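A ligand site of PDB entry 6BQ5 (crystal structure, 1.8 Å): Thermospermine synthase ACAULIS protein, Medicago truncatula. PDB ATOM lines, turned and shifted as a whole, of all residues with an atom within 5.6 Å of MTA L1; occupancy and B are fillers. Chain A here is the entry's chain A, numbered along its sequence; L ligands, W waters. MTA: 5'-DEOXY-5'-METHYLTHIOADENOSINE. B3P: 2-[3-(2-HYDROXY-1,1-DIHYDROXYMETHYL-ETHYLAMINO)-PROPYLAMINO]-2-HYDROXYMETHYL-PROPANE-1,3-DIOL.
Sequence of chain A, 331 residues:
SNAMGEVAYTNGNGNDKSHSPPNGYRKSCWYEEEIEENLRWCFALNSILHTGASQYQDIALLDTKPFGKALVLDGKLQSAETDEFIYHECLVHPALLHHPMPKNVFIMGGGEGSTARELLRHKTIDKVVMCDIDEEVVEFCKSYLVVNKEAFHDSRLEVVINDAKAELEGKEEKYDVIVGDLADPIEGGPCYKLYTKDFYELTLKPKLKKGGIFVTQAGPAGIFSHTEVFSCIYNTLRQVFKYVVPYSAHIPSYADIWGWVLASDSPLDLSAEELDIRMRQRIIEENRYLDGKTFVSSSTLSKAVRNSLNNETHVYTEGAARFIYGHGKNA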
ATOM      1  N   GLN A  57      16.138 -21.788   1.970  1.00  0.00           N
ATOM      2  CA  GLN A  57      16.385 -20.382   1.670  1.00  0.00           C
ATOM      3  C   GLN A  57      17.415 -19.692   2.580  1.00  0.00           C
ATOM      4  O   GLN A  57      17.734 -20.134   3.691  1.00  0.00           O
ATOM      5  CB  GLN A  57      15.032 -19.584   1.676  1.00  0.00           C
ATOM      6  CG  GLN A  57      14.316 -19.563   3.023  1.00  0.00           C
ATOM      7  CD  GLN A  57      12.803 -19.825   2.925  1.00  0.00           C
ATOM      8  OE1 GLN A  57      12.109 -19.268   2.060  1.00  0.00           O
ATOM      9  NE2 GLN A  57      12.293 -20.675   3.830  1.00  0.00           N
ATOM     10  N   LEU A  73      14.011 -13.065   2.385  1.00  0.00           N
ATOM     11  CA  LEU A  73      14.202 -14.489   2.118  1.00  0.00           C
ATOM     12  C   LEU A  73      14.621 -14.656   0.655  1.00  0.00           C
ATOM     13  O   LEU A  73      13.982 -14.141  -0.267  1.00  0.00           O
ATOM     14  CB  LEU A  73      12.921 -15.270   2.425  1.00  0.00           C
ATOM     15  CG  LEU A  73      12.363 -15.198   3.855  1.00  0.00           C
ATOM     16  CD1 LEU A  73      11.096 -16.030   3.972  1.00  0.00           C
ATOM     17  CD2 LEU A  73      13.353 -15.654   4.890  1.00  0.00           C
ATOM     18  N   GLN A  78      10.065  -9.814   2.309  1.00  0.00           N
ATOM     19  CA  GLN A  78       8.821 -10.477   2.801  1.00  0.00           C
ATOM     20  C   GLN A  78       7.921  -9.560   3.630  1.00  0.00           C
ATOM     21  O   GLN A  78       6.783  -9.328   3.255  1.00  0.00           O
ATOM     22  CB  GLN A  78       9.159 -11.704   3.607  1.00  0.00           C
ATOM     23  CG  GLN A  78      10.071 -12.694   2.864  1.00  0.00           C
ATOM     24  CD  GLN A  78       9.412 -13.267   1.626  1.00  0.00           C
ATOM     25  OE1 GLN A  78       8.298 -13.745   1.701  1.00  0.00           O
ATOM     26  NE2 GLN A  78      10.078 -13.201   0.471  1.00  0.00           N
ATOM     27  N   MET A 108      -0.878 -22.427   6.417  1.00  0.00           N
ATOM     28  CA  MET A 108       0.144 -22.940   5.494  1.00  0.00           C
ATOM     29  C   MET A 108       1.258 -21.880   5.323  1.00  0.00           C
ATOM     30  O   MET A 108       1.060 -20.806   4.651  1.00  0.00           O
ATOM     31  CB  MET A 108      -0.426 -23.355   4.125  1.00  0.00           C
ATOM     32  CG  MET A 108      -1.745 -24.132   4.193  1.00  0.00           C
ATOM     33  SD  MET A 108      -2.273 -24.811   2.614  1.00  0.00           S
ATOM     34  CE  MET A 108      -2.501 -23.300   1.671  1.00  0.00           C
ATOM     35  N   GLY A 109       2.407 -22.190   5.909  1.00  0.00           N
ATOM     36  CA  GLY A 109       3.537 -21.283   6.005  1.00  0.00           C
ATOM     37  C   GLY A 109       3.448 -20.501   7.300  1.00  0.00           C
ATOM     38  O   GLY A 109       3.160 -21.065   8.359  1.00  0.00           O
ATOM     39  N   GLY A 110       3.636 -19.191   7.209  1.00  0.00           N
ATOM     40  CA  GLY A 110       3.535 -18.354   8.403  1.00  0.00           C
ATOM     41  C   GLY A 110       4.660 -18.454   9.409  1.00  0.00           C
ATOM     42  O   GLY A 110       4.520 -17.967  10.557  1.00  0.00           O
ATOM     43  N   GLY A 111       5.812 -19.005   8.993  1.00  0.00           N
ATOM     44  CA  GLY A 111       6.970 -18.982   9.871  1.00  0.00           C
ATOM     45  C   GLY A 111       7.367 -17.615  10.418  1.00  0.00           C
ATOM     46  O   GLY A 111       7.966 -17.543  11.471  1.00  0.00           O
ATOM     47  N   GLU A 112       7.072 -16.546   9.686  1.00  0.00           N
ATOM     48  CA  GLU A 112       7.371 -15.192  10.123  1.00  0.00           C
ATOM     49  C   GLU A 112       6.615 -14.731  11.378  1.00  0.00           C
ATOM     50  O   GLU A 112       7.075 -13.871  12.110  1.00  0.00           O
ATOM     51  CB  GLU A 112       7.149 -14.250   8.925  1.00  0.00           C
ATOM     52  CG  GLU A 112       7.353 -12.753   9.147  1.00  0.00           C
ATOM     53  CD  GLU A 112       6.059 -11.972   9.428  1.00  0.00           C
ATOM     54  OE1 GLU A 112       6.107 -10.734   9.439  1.00  0.00           O
ATOM     55  OE2 GLU A 112       5.007 -12.612   9.610  1.00  0.00           O
ATOM     56  N   CYS A 131       1.995 -24.348  10.298  1.00  0.00           N
ATOM     57  CA  CYS A 131       2.749 -25.378   9.611  1.00  0.00           C
ATOM     58  C   CYS A 131       3.661 -24.758   8.541  1.00  0.00           C
ATOM     59  O   CYS A 131       3.217 -24.477   7.413  1.00  0.00           O
ATOM     60  CB  CYS A 131       1.804 -26.380   8.972  1.00  0.00           C
ATOM     61  SG  CYS A 131       2.641 -27.786   8.207  1.00  0.00           S
ATOM     62  N   ASP A 132       4.922 -24.516   8.914  1.00  0.00           N
ATOM     63  CA  ASP A 132       5.960 -24.003   7.992  1.00  0.00           C
ATOM     64  C   ASP A 132       7.015 -25.078   7.740  1.00  0.00           C
ATOM     65  O   ASP A 132       7.441 -25.758   8.662  1.00  0.00           O
ATOM     66  CB  ASP A 132       6.640 -22.776   8.587  1.00  0.00           C
ATOM     67  CG  ASP A 132       7.354 -21.936   7.529  1.00  0.00           C
ATOM     68  OD1 ASP A 132       8.334 -22.449   6.903  1.00  0.00           O
ATOM     69  OD2 ASP A 132       6.895 -20.786   7.289  1.00  0.00           O
ATOM     70  N   ILE A 133       7.408 -25.222   6.482  1.00  0.00           N
ATOM     71  CA  ILE A 133       8.384 -26.224   6.078  1.00  0.00           C
ATOM     72  C   ILE A 133       9.800 -25.949   6.597  1.00  0.00           C
ATOM     73  O   ILE A 133      10.581 -26.856   6.739  1.00  0.00           O
ATOM     74  CB  ILE A 133       8.399 -26.378   4.545  1.00  0.00           C
ATOM     75  CG1 ILE A 133       8.965 -27.730   4.114  1.00  0.00           C
ATOM     76  CG2 ILE A 133       9.099 -25.215   3.854  1.00  0.00           C
ATOM     77  CD1 ILE A 133       8.739 -27.976   2.642  1.00  0.00           C
ATOM     78  N   ASP A 134      10.107 -24.698   6.913  1.00  0.00           N
ATOM     79  CA  ASP A 134      11.472 -24.308   7.256  1.00  0.00           C
ATOM     80  C   ASP A 134      11.603 -23.852   8.727  1.00  0.00           C
ATOM     81  O   ASP A 134      11.369 -22.710   9.063  1.00  0.00           O
ATOM     82  CB  ASP A 134      11.927 -23.224   6.277  1.00  0.00           C
ATOM     83  CG  ASP A 134      13.402 -22.900   6.388  1.00  0.00           C
ATOM     84  OD1 ASP A 134      14.064 -23.447   7.298  1.00  0.00           O
ATOM     85  OD2 ASP A 134      13.898 -22.112   5.557  1.00  0.00           O
ATOM     86  N   VAL A 137      13.467 -20.546   9.456  1.00  0.00           N
ATOM     87  CA  VAL A 137      12.621 -19.324   9.339  1.00  0.00           C
ATOM     88  C   VAL A 137      11.884 -19.104  10.644  1.00  0.00           C
ATOM     89  O   VAL A 137      11.922 -18.009  11.210  1.00  0.00           O
ATOM     90  CB  VAL A 137      11.616 -19.418   8.189  1.00  0.00           C
ATOM     91  CG1 VAL A 137      10.587 -18.304   8.274  1.00  0.00           C
ATOM     92  CG2 VAL A 137      12.345 -19.361   6.860  1.00  0.00           C
ATOM     93  N   ASN A 162       6.693 -28.796   8.841  1.00  0.00           N
ATOM     94  CA  ASN A 162       6.409 -29.732   7.758  1.00  0.00           C
ATOM     95  C   ASN A 162       5.985 -29.050   6.457  1.00  0.00           C
ATOM     96  O   ASN A 162       5.644 -27.871   6.461  1.00  0.00           O
ATOM     97  CB  ASN A 162       5.309 -30.694   8.216  1.00  0.00           C
ATOM     98  CG  ASN A 162       5.259 -31.970   7.401  1.00  0.00           C
ATOM     99  OD1 ASN A 162       6.069 -32.216   6.506  1.00  0.00           O
ATOM    100  ND2 ASN A 162       4.274 -32.774   7.712  1.00  0.00           N
ATOM    101  N   ASP A 163       6.018 -29.781   5.349  1.00  0.00           N
ATOM    102  CA  ASP A 163       5.279 -29.378   4.161  1.00  0.00           C
ATOM    103  C   ASP A 163       3.754 -29.378   4.524  1.00  0.00           C
ATOM    104  O   ASP A 163       3.214 -30.363   5.007  1.00  0.00           O
ATOM    105  CB  ASP A 163       5.640 -30.283   2.964  1.00  0.00           C
ATOM    106  CG  ASP A 163       4.627 -30.213   1.841  1.00  0.00           C
ATOM    107  OD1 ASP A 163       4.129 -29.117   1.576  1.00  0.00           O
ATOM    108  OD2 ASP A 163       4.255 -31.274   1.296  1.00  0.00           O
ATOM    109  N   ALA A 164       3.073 -28.247   4.298  1.00  0.00           N
ATOM    110  CA  ALA A 164       1.662 -28.124   4.697  1.00  0.00           C
ATOM    111  C   ALA A 164       0.750 -29.085   3.922  1.00  0.00           C
ATOM    112  O   ALA A 164      -0.309 -29.451   4.426  1.00  0.00           O
ATOM    113  CB  ALA A 164       1.168 -26.683   4.542  1.00  0.00           C
ATOM    114  N   LYS A 165       1.135 -29.447   2.708  1.00  0.00           N
ATOM    115  CA  LYS A 165       0.382 -30.401   1.903  1.00  0.00           C
ATOM    116  C   LYS A 165       0.479 -31.799   2.551  1.00  0.00           C
ATOM    117  O   LYS A 165      -0.558 -32.389   2.874  1.00  0.00           O
ATOM    118  CB  LYS A 165       0.895 -30.415   0.455  1.00  0.00           C
ATOM    119  CG  LYS A 165       0.236 -31.442  -0.479  1.00  0.00           C
ATOM    120  CD  LYS A 165       0.808 -31.332  -1.904  1.00  0.00           C
ATOM    121  CE  LYS A 165      -0.077 -32.053  -2.926  1.00  0.00           C
ATOM    122  NZ  LYS A 165      -0.347 -33.462  -2.509  1.00  0.00           N
ATOM    123  N   ASP A 181      -0.359 -18.763   3.395  1.00  0.00           N
ATOM    124  CA  ASP A 181       0.622 -17.690   3.585  1.00  0.00           C
ATOM    125  C   ASP A 181       1.937 -18.115   2.939  1.00  0.00           C
ATOM    126  O   ASP A 181       3.032 -17.914   3.504  1.00  0.00           O
ATOM    127  CB  ASP A 181       0.765 -17.411   5.079  1.00  0.00           C
ATOM    128  CG  ASP A 181       1.490 -16.101   5.440  1.00  0.00           C
ATOM    129  OD1 ASP A 181       1.738 -15.238   4.540  1.00  0.00           O
ATOM    130  OD2 ASP A 181       1.781 -15.944   6.651  1.00  0.00           O
ATOM    131  N   LEU A 182       1.830 -18.645   1.731  1.00  0.00           N
ATOM    132  CA  LEU A 182       2.971 -19.164   0.991  1.00  0.00           C
ATOM    133  C   LEU A 182       3.501 -18.184  -0.043  1.00  0.00           C
ATOM    134  O   LEU A 182       2.944 -17.078  -0.246  1.00  0.00           O
ATOM    135  CB  LEU A 182       2.570 -20.472   0.296  1.00  0.00           C
ATOM    136  CG  LEU A 182       2.115 -21.608   1.199  1.00  0.00           C
ATOM    137  CD1 LEU A 182       1.246 -22.639   0.470  1.00  0.00           C
ATOM    138  CD2 LEU A 182       3.266 -22.297   1.888  1.00  0.00           C
ATOM    139  N   ALA A 183       4.600 -18.583  -0.707  1.00  0.00           N
ATOM    140  CA  ALA A 183       5.074 -17.948  -1.898  1.00  0.00           C
ATOM    141  C   ALA A 183       4.094 -18.150  -3.059  1.00  0.00           C
ATOM    142  O   ALA A 183       3.241 -19.012  -3.056  1.00  0.00           O
ATOM    143  CB  ALA A 183       6.490 -18.436  -2.300  1.00  0.00           C
ATOM    144  N   PRO A 190       8.600 -24.695  -5.291  1.00  0.00           N
ATOM    145  CA  PRO A 190       8.217 -25.483  -4.125  1.00  0.00           C
ATOM    146  C   PRO A 190       6.758 -25.308  -3.674  1.00  0.00           C
ATOM    147  O   PRO A 190       6.207 -26.230  -3.029  1.00  0.00           O
ATOM    148  CB  PRO A 190       9.136 -24.935  -3.031  1.00  0.00           C
ATOM    149  CG  PRO A 190       9.363 -23.521  -3.409  1.00  0.00           C
ATOM    150  CD  PRO A 190       9.401 -23.516  -4.918  1.00  0.00           C
ATOM    151  N   CYS A 191       6.163 -24.143  -3.953  1.00  0.00           N
ATOM    152  CA  CYS A 191       4.795 -23.831  -3.469  1.00  0.00           C
ATOM    153  C   CYS A 191       3.681 -24.103  -4.498  1.00  0.00           C
ATOM    154  O   CYS A 191       2.500 -24.101  -4.129  1.00  0.00           O
ATOM    155  CB  CYS A 191       4.737 -22.369  -2.976  1.00  0.00           C
ATOM    156  SG  CYS A 191       5.752 -22.064  -1.478  1.00  0.00           S
ATOM    157  N   LYS A 193       2.378 -26.599  -5.990  1.00  0.00           N
ATOM    158  CA  LYS A 193       1.446 -27.673  -5.722  1.00  0.00           C
ATOM    159  C   LYS A 193       0.388 -27.329  -4.673  1.00  0.00           C
ATOM    160  O   LYS A 193      -0.560 -28.088  -4.522  1.00  0.00           O
ATOM    161  CB  LYS A 193       2.207 -28.952  -5.309  1.00  0.00           C
ATOM    162  CG  LYS A 193       2.819 -28.840  -3.921  1.00  0.00           C
ATOM    163  CD  LYS A 193       3.987 -29.779  -3.665  1.00  0.00           C
ATOM    164  CE  LYS A 193       4.433 -29.640  -2.216  1.00  0.00           C
ATOM    165  NZ  LYS A 193       5.153 -30.869  -1.764  1.00  0.00           N
ATOM    166  N   LEU A 194       0.574 -26.256  -3.901  1.00  0.00           N
ATOM    167  CA  LEU A 194      -0.429 -25.819  -2.903  1.00  0.00           C
ATOM    168  C   LEU A 194      -1.421 -24.777  -3.480  1.00  0.00           C
ATOM    169  O   LEU A 194      -2.120 -24.150  -2.699  1.00  0.00           O
ATOM    170  CB  LEU A 194       0.245 -25.320  -1.612  1.00  0.00           C
ATOM    171  CG  LEU A 194       1.039 -26.403  -0.849  1.00  0.00           C
ATOM    172  CD1 LEU A 194       2.519 -26.352  -1.194  1.00  0.00           C
ATOM    173  CD2 LEU A 194       0.871 -26.360   0.671  1.00  0.00           C
HETATM  174  CS  MTA L   1       8.320 -16.824   1.511  1.00  0.00           C
HETATM  175  S5' MTA L   1       7.479 -18.356   1.470  1.00  0.00           S
HETATM  176  C5' MTA L   1       6.478 -18.118   2.901  1.00  0.00           C
HETATM  177  C4' MTA L   1       6.692 -19.272   3.885  1.00  0.00           C
HETATM  178  O4' MTA L   1       6.273 -20.495   3.299  1.00  0.00           O
HETATM  179  C2' MTA L   1       8.510 -20.862   3.823  1.00  0.00           C
HETATM  180  O2' MTA L   1       9.396 -21.474   4.758  1.00  0.00           O
HETATM  181  C3' MTA L   1       8.159 -19.472   4.267  1.00  0.00           C
HETATM  182  O3' MTA L   1       8.288 -19.247   5.665  1.00  0.00           O
HETATM  183  C1' MTA L   1       7.156 -21.527   3.779  1.00  0.00           C
HETATM  184  N9  MTA L   1       6.917 -22.631   2.853  1.00  0.00           N
HETATM  185  C8  MTA L   1       7.330 -22.786   1.586  1.00  0.00           C
HETATM  186  N7  MTA L   1       6.830 -23.930   1.056  1.00  0.00           N
HETATM  187  C5  MTA L   1       6.067 -24.492   2.008  1.00  0.00           C
HETATM  188  C6  MTA L   1       5.276 -25.719   2.110  1.00  0.00           C
HETATM  189  N6  MTA L   1       5.172 -26.564   1.054  1.00  0.00           N
HETATM  190  N1  MTA L   1       4.623 -25.938   3.265  1.00  0.00           N
HETATM  191  C2  MTA L   1       4.727 -25.093   4.321  1.00  0.00           C
HETATM  192  N3  MTA L   1       5.438 -23.951   4.305  1.00  0.00           N
HETATM  193  C4  MTA L   1       6.126 -23.644   3.181  1.00  0.00           C
HETATM  194  C1  B3P L   2       7.029 -11.676  -1.058  1.00  0.00           C
HETATM  195  C2  B3P L   2       6.914 -10.347  -1.783  1.00  0.00           C
HETATM  196  C3  B3P L   2       5.682 -11.937  -0.386  1.00  0.00           C
HETATM  197  N1  B3P L   2       5.715 -13.103   0.491  1.00  0.00           N
HETATM  198  C4  B3P L   2       4.551 -13.479   1.283  1.00  0.00           C
HETATM  199  C5  B3P L   2       4.959 -14.765   2.038  1.00  0.00           C
HETATM  200  C6  B3P L   2       4.187 -12.342   2.232  1.00  0.00           C
HETATM  201  C7  B3P L   2       3.345 -13.718   0.366  1.00  0.00           C
HETATM  202  N2  B3P L   2       8.108 -10.051  -2.544  1.00  0.00           N
HETATM  203  C8  B3P L   2       8.179  -8.923  -3.444  1.00  0.00           C
HETATM  204  C9  B3P L   2       9.595  -8.963  -4.026  1.00  0.00           C
HETATM  205  C10 B3P L   2       7.891  -7.617  -2.673  1.00  0.00           C
HETATM  206  C11 B3P L   2       7.181  -9.061  -4.598  1.00  0.00           C
HETATM  207  O1  B3P L   2      10.542  -9.029  -2.960  1.00  0.00           O
HETATM  208  O2  B3P L   2       8.052  -6.505  -3.558  1.00  0.00           O
HETATM  209  O3  B3P L   2       7.125 -10.399  -5.095  1.00  0.00           O
HETATM  210  O4  B3P L   2       3.885 -15.280   2.812  1.00  0.00           O
HETATM  211  O5  B3P L   2       5.357 -11.800   2.852  1.00  0.00           O
HETATM  212  O6  B3P L   2       3.603 -14.646  -0.714  1.00  0.00           O
HETATM  213  O   HOH W   1       7.050 -16.808   6.521  1.00  0.00           O
HETATM  214  O   HOH W   2       6.838 -15.019  -0.970  1.00  0.00           O
HETATM  215  O   HOH W   3       4.614 -16.828   5.528  1.00  0.00           O
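The side-chain carboxylate of Asp 132 lies within hydrogen-bond range of an oxygen (O2') of MTA L1 (2.6 Å).
The side-chain carboxylate (OD1) of Asp 163 is in hydrogen-bond range of a nitrogen (N6) of MTA L1 (2.8 Å).
N of Ala 164 lies within hydrogen-bond range of N1 of MTA L1.
NE2 of Gln 57 sits at hydrogen-bond distance from O2' of MTA L1 (3.1 Å).
The backbone NH (N) of Ile 133 lies within hydrogen-bond range of a nitrogen (N3) of MTA L1 (3.2 Å).
The side-chain sulfur (SG) of Cys 191 sits at hydrogen-bond distance from a nitrogen (N7) of MTA L1.
A sulfur (S5') of MTA L1 sits close to the backbone NH (N) of Ala 183.
An oxygen (O5) of B3P L2 sits at hydrogen-bond distance from the backbone carbonyl oxygen of Gln 78, at 2.9 Å.
The side-chain amide oxygen of Gln 78 lies within hydrogen-bond range of a nitrogen (N1) of B3P L2, 2.9 Å away.
An oxygen (O6) of B3P L2 is in hydrogen-bond range of the backbone carbonyl oxygen of Leu 182.
The backbone carbonyl oxygen (O) of Asp 181 sits at hydrogen-bond distance from an oxygen (O4) of B3P L2 (2.9 Å).
OD1 of Asp 181 is in hydrogen-bond range of O4 of B3P L2 (2.8 Å).
The side-chain carboxylate (OD1) of Asp 132 is in hydrogen-bond range of the backbone NH (N) of Asp 134, at 2.9 Å.
The backbone NH (N) of Asn 162 sits at hydrogen-bond distance from the backbone carbonyl oxygen (O) of Asp 132 (3.1 Å).
The side-chain carboxylate of Asp 163 lies within salt-bridge range of the side-chain amino group of Lys 193, 3.2 Å away.
The side-chain amide nitrogen (NE2) of Gln 57 is in hydrogen-bond range of the side-chain carboxylate (OD2) of Asp 134 (2.8 Å).
The side-chain sulfur (SG) of Cys 191 is in hydrogen-bond range of the backbone NH (N) of Ala 183 (3.7 Å).
The side-chain sulfur (SG) of Cys 131 is in hydrogen-bond range of the backbone carbonyl oxygen (O) of Asn 162 (3.5 Å).
The backbone carbonyl oxygen of Cys 131 lies within hydrogen-bond range of the backbone NH of Gly 109, at 2.9 Å.
N of Asp 181 lies within hydrogen-bond range of O of Met 108, at 2.8 Å.
Residues that only touch MTA L1: Gln 78, Leu 182, Asp 134, Leu 194, Cys 131, Asp 181, Val 137, Asn 162, Gly 109 and Leu 73.
Hydrophobic or aromatic side chains that line MTA L1: Leu 73, Ile 133, Val 137, Ala 164, Leu 182, Ala 183 and Leu 194.
The nearest printed residue that does not touch MTA L1 is Gly 111 (4.2 Å).
Water W1 bridges O3' of MTA L1 (2.9 Å) and N of Glu 112 (3.2 Å).
Water W2 lies within hydrogen-bond range of N1 of B3P L2 (2.7 Å) and OE1 of Gln 78 (3.3 Å).
Water W3 lies within hydrogen-bond range of the backbone carbonyl oxygen (O) of Asp 181 (2.8 Å), the backbone NH (N) of Gly 110 (3.1 Å) and an oxygen (O4) of B3P L2 (3.2 Å).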
